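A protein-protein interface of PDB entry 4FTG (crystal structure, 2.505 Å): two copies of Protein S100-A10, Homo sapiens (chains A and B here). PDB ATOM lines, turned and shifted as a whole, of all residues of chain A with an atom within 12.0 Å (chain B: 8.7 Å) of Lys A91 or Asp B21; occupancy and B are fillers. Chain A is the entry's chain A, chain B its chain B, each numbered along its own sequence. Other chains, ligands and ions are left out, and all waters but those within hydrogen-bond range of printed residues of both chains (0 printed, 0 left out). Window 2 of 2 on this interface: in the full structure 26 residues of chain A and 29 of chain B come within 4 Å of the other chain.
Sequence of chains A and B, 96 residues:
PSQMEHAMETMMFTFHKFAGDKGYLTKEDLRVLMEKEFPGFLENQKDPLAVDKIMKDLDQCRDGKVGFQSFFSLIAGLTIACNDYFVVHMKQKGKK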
ATOM      1  N   ILE A  80      15.283  16.647  13.220  1.00  0.00           N
ATOM      2  CA  ILE A  80      14.071  17.411  13.398  1.00  0.00           C
ATOM      3  C   ILE A  80      13.407  17.703  12.057  1.00  0.00           C
ATOM      4  O   ILE A  80      12.185  17.665  11.960  1.00  0.00           O
ATOM      5  CB  ILE A  80      14.374  18.689  14.190  1.00  0.00           C
ATOM      6  CG1 ILE A  80      14.625  18.322  15.665  1.00  0.00           C
ATOM      7  CG2 ILE A  80      13.251  19.728  14.059  1.00  0.00           C
ATOM      8  CD1 ILE A  80      15.335  19.401  16.440  1.00  0.00           C
ATOM      9  N   ALA A  81      14.203  17.963  11.018  1.00  0.00           N
ATOM     10  CA  ALA A  81      13.643  18.141   9.673  1.00  0.00           C
ATOM     11  C   ALA A  81      13.030  16.848   9.155  1.00  0.00           C
ATOM     12  O   ALA A  81      11.945  16.879   8.585  1.00  0.00           O
ATOM     13  CB  ALA A  81      14.686  18.696   8.683  1.00  0.00           C
ATOM     14  N   CYS A  82      13.703  15.716   9.371  1.00  0.00           N
ATOM     15  CA  CYS A  82      13.128  14.413   9.022  1.00  0.00           C
ATOM     16  C   CYS A  82      11.794  14.176   9.699  1.00  0.00           C
ATOM     17  O   CYS A  82      10.833  13.729   9.075  1.00  0.00           O
ATOM     18  CB  CYS A  82      14.056  13.277   9.421  1.00  0.00           C
ATOM     19  SG  CYS A  82      15.490  13.217   8.379  1.00  0.00           S
ATOM     20  N   ASN A  83      11.745  14.476  10.987  1.00  0.00           N
ATOM     21  CA  ASN A  83      10.544  14.227  11.748  1.00  0.00           C
ATOM     22  C   ASN A  83       9.419  15.136  11.274  1.00  0.00           C
ATOM     23  O   ASN A  83       8.273  14.724  11.197  1.00  0.00           O
ATOM     24  CB  ASN A  83      10.799  14.425  13.235  1.00  0.00           C
ATOM     25  CG  ASN A  83       9.537  14.267  14.058  1.00  0.00           C
ATOM     26  OD1 ASN A  83       9.034  13.144  14.247  1.00  0.00           O
ATOM     27  ND2 ASN A  83       9.003  15.388  14.536  1.00  0.00           N
ATOM     28  N   ASP A  84       9.755  16.378  10.951  1.00  0.00           N
ATOM     29  CA  ASP A  84       8.780  17.310  10.387  1.00  0.00           C
ATOM     30  C   ASP A  84       8.163  16.763   9.101  1.00  0.00           C
ATOM     31  O   ASP A  84       6.941  16.668   8.987  1.00  0.00           O
ATOM     32  CB  ASP A  84       9.416  18.678  10.144  1.00  0.00           C
ATOM     33  CG  ASP A  84       9.488  19.522  11.414  1.00  0.00           C
ATOM     34  OD1 ASP A  84       8.873  19.113  12.447  1.00  0.00           O
ATOM     35  OD2 ASP A  84      10.154  20.590  11.368  1.00  0.00           O
ATOM     36  N   TYR A  85       9.017  16.379   8.156  1.00  0.00           N
ATOM     37  CA  TYR A  85       8.575  15.732   6.931  1.00  0.00           C
ATOM     38  C   TYR A  85       7.789  14.464   7.246  1.00  0.00           C
ATOM     39  O   TYR A  85       6.759  14.197   6.633  1.00  0.00           O
ATOM     40  CB  TYR A  85       9.779  15.420   6.037  1.00  0.00           C
ATOM     41  CG  TYR A  85       9.418  14.861   4.685  1.00  0.00           C
ATOM     42  CD1 TYR A  85       9.118  13.521   4.529  1.00  0.00           C
ATOM     43  CD2 TYR A  85       9.398  15.666   3.565  1.00  0.00           C
ATOM     44  CE1 TYR A  85       8.790  12.993   3.305  1.00  0.00           C
ATOM     45  CE2 TYR A  85       9.076  15.143   2.324  1.00  0.00           C
ATOM     46  CZ  TYR A  85       8.772  13.801   2.204  1.00  0.00           C
ATOM     47  OH  TYR A  85       8.437  13.249   0.985  1.00  0.00           O
ATOM     48  N   PHE A  86       8.281  13.684   8.202  1.00  0.00           N
ATOM     49  CA  PHE A  86       7.621  12.441   8.606  1.00  0.00           C
ATOM     50  C   PHE A  86       6.167  12.655   9.000  1.00  0.00           C
ATOM     51  O   PHE A  86       5.264  12.010   8.477  1.00  0.00           O
ATOM     52  CB  PHE A  86       8.329  11.853   9.806  1.00  0.00           C
ATOM     53  CG  PHE A  86       7.710  10.576  10.307  1.00  0.00           C
ATOM     54  CD1 PHE A  86       7.795   9.419   9.566  1.00  0.00           C
ATOM     55  CD2 PHE A  86       7.077  10.534  11.533  1.00  0.00           C
ATOM     56  CE1 PHE A  86       7.251   8.260  10.019  1.00  0.00           C
ATOM     57  CE2 PHE A  86       6.519   9.365  11.990  1.00  0.00           C
ATOM     58  CZ  PHE A  86       6.608   8.222  11.228  1.00  0.00           C
ATOM     59  N   VAL A  87       5.955  13.553   9.949  1.00  0.00           N
ATOM     60  CA  VAL A  87       4.612  13.900  10.371  1.00  0.00           C
ATOM     61  C   VAL A  87       3.744  14.350   9.190  1.00  0.00           C
ATOM     62  O   VAL A  87       2.672  13.794   8.972  1.00  0.00           O
ATOM     63  CB  VAL A  87       4.628  14.982  11.453  1.00  0.00           C
ATOM     64  CG1 VAL A  87       3.223  15.333  11.829  1.00  0.00           C
ATOM     65  CG2 VAL A  87       5.389  14.484  12.661  1.00  0.00           C
ATOM     66  N   VAL A  88       4.216  15.324   8.417  1.00  0.00           N
ATOM     67  CA  VAL A  88       3.416  15.859   7.322  1.00  0.00           C
ATOM     68  C   VAL A  88       2.993  14.801   6.288  1.00  0.00           C
ATOM     69  O   VAL A  88       1.811  14.708   5.958  1.00  0.00           O
ATOM     70  CB  VAL A  88       4.134  17.009   6.578  1.00  0.00           C
ATOM     71  CG1 VAL A  88       3.345  17.397   5.315  1.00  0.00           C
ATOM     72  CG2 VAL A  88       4.365  18.220   7.506  1.00  0.00           C
ATOM     73  N   HIS A  89       3.947  14.010   5.783  1.00  0.00           N
ATOM     74  CA  HIS A  89       3.686  13.121   4.639  1.00  0.00           C
ATOM     75  C   HIS A  89       3.575  11.642   4.968  1.00  0.00           C
ATOM     76  O   HIS A  89       3.119  10.866   4.134  1.00  0.00           O
ATOM     77  CB  HIS A  89       4.775  13.244   3.573  1.00  0.00           C
ATOM     78  CG  HIS A  89       4.995  14.635   3.079  1.00  0.00           C
ATOM     79  ND1 HIS A  89       5.888  15.502   3.672  1.00  0.00           N
ATOM     80  CD2 HIS A  89       4.448  15.310   2.043  1.00  0.00           C
ATOM     81  CE1 HIS A  89       5.881  16.652   3.020  1.00  0.00           C
ATOM     82  NE2 HIS A  89       5.009  16.563   2.032  1.00  0.00           N
ATOM     83  N   MET A  90       4.019  11.233   6.150  1.00  0.00           N
ATOM     84  CA  MET A  90       4.186   9.803   6.397  1.00  0.00           C
ATOM     85  C   MET A  90       3.432   9.187   7.569  1.00  0.00           C
ATOM     86  O   MET A  90       3.065   8.029   7.501  1.00  0.00           O
ATOM     87  CB  MET A  90       5.669   9.462   6.490  1.00  0.00           C
ATOM     88  CG  MET A  90       6.374   9.540   5.157  1.00  0.00           C
ATOM     89  SD  MET A  90       8.105   9.128   5.360  1.00  0.00           S
ATOM     90  CE  MET A  90       8.522   8.522   3.721  1.00  0.00           C
ATOM     91  N   LYS A  91       3.208   9.938   8.641  1.00  0.00           N
ATOM     92  CA  LYS A  91       2.520   9.388   9.811  1.00  0.00           C
ATOM     93  C   LYS A  91       1.008   9.403   9.612  1.00  0.00           C
ATOM     94  O   LYS A  91       0.359   8.356   9.646  1.00  0.00           O
ATOM     95  CB  LYS A  91       2.895  10.170  11.071  1.00  0.00           C
ATOM     96  CG  LYS A  91       2.309   9.629  12.371  1.00  0.00           C
ATOM     97  CD  LYS A  91       2.507  10.635  13.514  1.00  0.00           C
ATOM     98  CE  LYS A  91       2.182  10.045  14.883  1.00  0.00           C
ATOM     99  NZ  LYS A  91       2.387  11.054  15.960  1.00  0.00           N
ATOM    100  N   MET B  12      13.541   8.964  16.463  1.00  0.00           N
ATOM    101  CA  MET B  12      12.295   9.437  15.873  1.00  0.00           C
ATOM    102  C   MET B  12      11.188   8.456  16.194  1.00  0.00           C
ATOM    103  O   MET B  12      10.085   8.851  16.598  1.00  0.00           O
ATOM    104  CB  MET B  12      12.449   9.569  14.364  1.00  0.00           C
ATOM    105  CG  MET B  12      11.531  10.570  13.690  1.00  0.00           C
ATOM    106  SD  MET B  12      11.870  10.662  11.904  1.00  0.00           S
ATOM    107  CE  MET B  12      10.821   9.374  11.286  1.00  0.00           C
ATOM    108  N   PHE B  13      11.481   7.168  16.050  1.00  0.00           N
ATOM    109  CA  PHE B  13      10.454   6.147  16.322  1.00  0.00           C
ATOM    110  C   PHE B  13      10.141   6.004  17.822  1.00  0.00           C
ATOM    111  O   PHE B  13       8.981   5.807  18.210  1.00  0.00           O
ATOM    112  CB  PHE B  13      10.794   4.803  15.661  1.00  0.00           C
ATOM    113  CG  PHE B  13      10.578   4.790  14.145  1.00  0.00           C
ATOM    114  CD1 PHE B  13      10.064   5.910  13.483  1.00  0.00           C
ATOM    115  CD2 PHE B  13      10.875   3.653  13.383  1.00  0.00           C
ATOM    116  CE1 PHE B  13       9.860   5.898  12.094  1.00  0.00           C
ATOM    117  CE2 PHE B  13      10.674   3.633  11.996  1.00  0.00           C
ATOM    118  CZ  PHE B  13      10.168   4.759  11.352  1.00  0.00           C
ATOM    119  N   PHE B  15      10.221   8.484  19.967  1.00  0.00           N
ATOM    120  CA  PHE B  15       9.344   9.595  20.338  1.00  0.00           C
ATOM    121  C   PHE B  15       7.897   9.257  20.037  1.00  0.00           C
ATOM    122  O   PHE B  15       7.032   9.355  20.908  1.00  0.00           O
ATOM    123  CB  PHE B  15       9.715  10.888  19.624  1.00  0.00           C
ATOM    124  CG  PHE B  15       8.734  12.033  19.870  1.00  0.00           C
ATOM    125  CD1 PHE B  15       7.761  12.357  18.918  1.00  0.00           C
ATOM    126  CD2 PHE B  15       8.792  12.784  21.042  1.00  0.00           C
ATOM    127  CE1 PHE B  15       6.857  13.402  19.120  1.00  0.00           C
ATOM    128  CE2 PHE B  15       7.890  13.847  21.251  1.00  0.00           C
ATOM    129  CZ  PHE B  15       6.923  14.152  20.290  1.00  0.00           C
ATOM    130  N   HIS B  16       7.638   8.847  18.800  1.00  0.00           N
ATOM    131  CA  HIS B  16       6.279   8.560  18.408  1.00  0.00           C
ATOM    132  C   HIS B  16       5.680   7.380  19.162  1.00  0.00           C
ATOM    133  O   HIS B  16       4.480   7.341  19.384  1.00  0.00           O
ATOM    134  CB  HIS B  16       6.185   8.414  16.895  1.00  0.00           C
ATOM    135  CG  HIS B  16       6.336   9.726  16.188  1.00  0.00           C
ATOM    136  ND1 HIS B  16       5.388  10.722  16.274  1.00  0.00           N
ATOM    137  CD2 HIS B  16       7.346  10.228  15.445  1.00  0.00           C
ATOM    138  CE1 HIS B  16       5.802  11.777  15.591  1.00  0.00           C
ATOM    139  NE2 HIS B  16       6.992  11.502  15.084  1.00  0.00           N
ATOM    140  N   LYS B  17       6.520   6.438  19.582  1.00  0.00           N
ATOM    141  CA  LYS B  17       6.027   5.272  20.301  1.00  0.00           C
ATOM    142  C   LYS B  17       5.378   5.674  21.635  1.00  0.00           C
ATOM    143  O   LYS B  17       4.342   5.144  22.010  1.00  0.00           O
ATOM    144  CB  LYS B  17       7.156   4.270  20.521  1.00  0.00           C
ATOM    145  CG  LYS B  17       6.754   3.032  21.308  1.00  0.00           C
ATOM    146  CD  LYS B  17       7.958   2.144  21.612  1.00  0.00           C
ATOM    147  CE  LYS B  17       7.575   1.034  22.575  1.00  0.00           C
ATOM    148  NZ  LYS B  17       8.667   0.017  22.699  1.00  0.00           N
ATOM    149  N   PHE B  18       5.974   6.633  22.333  1.00  0.00           N
ATOM    150  CA  PHE B  18       5.501   7.021  23.663  1.00  0.00           C
ATOM    151  C   PHE B  18       4.603   8.254  23.680  1.00  0.00           C
ATOM    152  O   PHE B  18       3.964   8.539  24.689  1.00  0.00           O
ATOM    153  CB  PHE B  18       6.685   7.228  24.609  1.00  0.00           C
ATOM    154  CG  PHE B  18       7.350   5.955  25.016  1.00  0.00           C
ATOM    155  CD1 PHE B  18       6.823   5.181  26.036  1.00  0.00           C
ATOM    156  CD2 PHE B  18       8.487   5.514  24.365  1.00  0.00           C
ATOM    157  CE1 PHE B  18       7.431   3.990  26.409  1.00  0.00           C
ATOM    158  CE2 PHE B  18       9.105   4.330  24.733  1.00  0.00           C
ATOM    159  CZ  PHE B  18       8.575   3.567  25.754  1.00  0.00           C
ATOM    160  N   ALA B  19       4.564   8.978  22.568  1.00  0.00           N
ATOM    161  CA  ALA B  19       3.776  10.195  22.457  1.00  0.00           C
ATOM    162  C   ALA B  19       2.408   9.918  21.832  1.00  0.00           C
ATOM    163  O   ALA B  19       1.448  10.660  22.074  1.00  0.00           O
ATOM    164  CB  ALA B  19       4.521  11.224  21.625  1.00  0.00           C
ATOM    165  N   GLY B  20       2.340   8.875  21.002  1.00  0.00           N
ATOM    166  CA  GLY B  20       1.112   8.492  20.322  1.00  0.00           C
ATOM    167  C   GLY B  20       0.678   9.447  19.231  1.00  0.00           C
ATOM    168  O   GLY B  20       1.423  10.347  18.838  1.00  0.00           O
ATOM    169  N   ASP B  21      -0.540   9.260  18.740  1.00  0.00           N
ATOM    170  CA  ASP B  21      -1.086  10.141  17.710  1.00  0.00           C
ATOM    171  C   ASP B  21      -1.205  11.594  18.170  1.00  0.00           C
ATOM    172  O   ASP B  21      -1.179  12.502  17.347  1.00  0.00           O
ATOM    173  CB  ASP B  21      -2.441   9.634  17.226  1.00  0.00           C
ATOM    174  CG  ASP B  21      -2.348   8.282  16.566  1.00  0.00           C
ATOM    175  OD1 ASP B  21      -2.580   7.267  17.251  1.00  0.00           O
ATOM    176  OD2 ASP B  21      -2.040   8.229  15.360  1.00  0.00           O
ATOM    177  N   LYS B  22      -1.328  11.817  19.477  1.00  0.00           N
ATOM    178  CA  LYS B  22      -1.327  13.178  20.005  1.00  0.00           C
ATOM    179  C   LYS B  22      -0.081  13.981  19.570  1.00  0.00           C
ATOM    180  O   LYS B  22      -0.087  15.216  19.586  1.00  0.00           O
ATOM    181  CB  LYS B  22      -1.490  13.166  21.528  1.00  0.00           C
ATOM    182  CG  LYS B  22      -2.812  12.545  21.968  1.00  0.00           C
ATOM    183  CD  LYS B  22      -3.213  12.946  23.388  1.00  0.00           C
ATOM    184  CE  LYS B  22      -4.715  12.737  23.637  1.00  0.00           C
ATOM    185  NZ  LYS B  22      -5.104  13.015  25.052  1.00  0.00           N
ATOM    186  N   GLY B  23       0.980  13.277  19.181  1.00  0.00           N
ATOM    187  CA  GLY B  23       2.138  13.913  18.582  1.00  0.00           C
ATOM    188  C   GLY B  23       2.987  14.697  19.560  1.00  0.00           C
ATOM    189  O   GLY B  23       3.764  15.574  19.160  1.00  0.00           O
ATOM    190  N   TYR B  24       2.835  14.375  20.842  1.00  0.00           N
ATOM    191  CA  TYR B  24       3.629  14.994  21.895  1.00  0.00           C
ATOM    192  C   TYR B  24       3.604  14.156  23.185  1.00  0.00           C
ATOM    193  O   TYR B  24       2.855  13.186  23.307  1.00  0.00           O
ATOM    194  CB  TYR B  24       3.177  16.438  22.167  1.00  0.00           C
ATOM    195  CG  TYR B  24       1.859  16.545  22.907  1.00  0.00           C
ATOM    196  CD1 TYR B  24       1.814  16.511  24.297  1.00  0.00           C
ATOM    197  CD2 TYR B  24       0.662  16.673  22.214  1.00  0.00           C
ATOM    198  CE1 TYR B  24       0.611  16.593  24.978  1.00  0.00           C
ATOM    199  CE2 TYR B  24      -0.535  16.761  22.874  1.00  0.00           C
ATOM    200  CZ  TYR B  24      -0.559  16.726  24.258  1.00  0.00           C
ATOM    201  OH  TYR B  24      -1.757  16.814  24.926  1.00  0.00           O
ATOM    202  N   ASP B  29       3.942  10.357  29.818  1.00  0.00           N
ATOM    203  CA  ASP B  29       4.572   9.749  28.655  1.00  0.00           C
ATOM    204  C   ASP B  29       6.070   9.773  28.873  1.00  0.00           C
ATOM    205  O   ASP B  29       6.736   8.730  28.790  1.00  0.00           O
ATOM    206  CB  ASP B  29       4.221  10.520  27.391  1.00  0.00           C
ATOM    207  CG  ASP B  29       2.734  10.535  27.119  1.00  0.00           C
ATOM    208  OD1 ASP B  29       2.067   9.557  27.497  1.00  0.00           O
ATOM    209  OD2 ASP B  29       2.235  11.524  26.530  1.00  0.00           O
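The backbone NH (N) of Lys A91 sits at hydrogen-bond distance from the backbone carbonyl oxygen (O) of Phe A86 (2.9 Å).
Among the printed residues, pairs that only touch across the chains: Phe A86 with Met B12, Asn A83 with Met B12, Phe A86 with His B16, Lys A91 with Gly B23 and Lys A91 with Asp B21.
No position is printed for both chains.
Of the printed residues of chain B, Asn A83 touches Met B12 and His B16.
Of the printed residues of chain B, Phe A86 touches Met B12 and His B16.
Printed residues of chain B within 4 Å of Lys A91: His B16 (3.0 Å), Gly B20 (3.1 Å), Asp B21 (3.99 Å) and Gly B23 (3.9 Å).
Printed residues of chain A within 4 Å of Met B12: Asn A83 and Phe A86.
Of the printed residues of chain A, His B16 touches Asn A83 (2.8 Å), Phe A86 (3.7 Å) and Lys A91 (3.0 Å).
Phe B18 touches none of the printed residues of chain A.
No residue of chain A comes within 4 Å of Ala B19.
Gly B20 touches one residue of chain A.
Of the printed residues of chain A, Asp B21 touches Lys A91.
Of chain A, only Lys A91 (3.9 Å) comes within 4 Å of Gly B23.
Tyr B24 touches none of the printed residues of chain A.
The nearest printed residue of chain B that does not touch Phe A86 is Phe B13 (4.1 Å).
NE2 of His B16 is in hydrogen-bond range of OD1 of Asn A83, 2.8 Å away.
The side-chain amino group of Lys A91 sits at hydrogen-bond distance from a ring nitrogen (ND1) of His B16 (3.0 Å).
O of Gly B20 is in hydrogen-bond range of NZ of Lys A91 (3.1 Å).
Hydrophobic or aromatic side chains of chain B within 4 Å of the printed part of chain A: Met B12 and His B16.
Of the 12 printed residues of chain A, 3 touch a printed residue of chain B.
Printed residues of chain A that touch a printed residue of chain B: Asn A83, Phe A86 and Lys A91.
Hydrophobic or aromatic side chains of chain A within 4 Å of the printed part of chain B: Phe A86.
Among the printed residues, 8 pairs touch across the chains.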
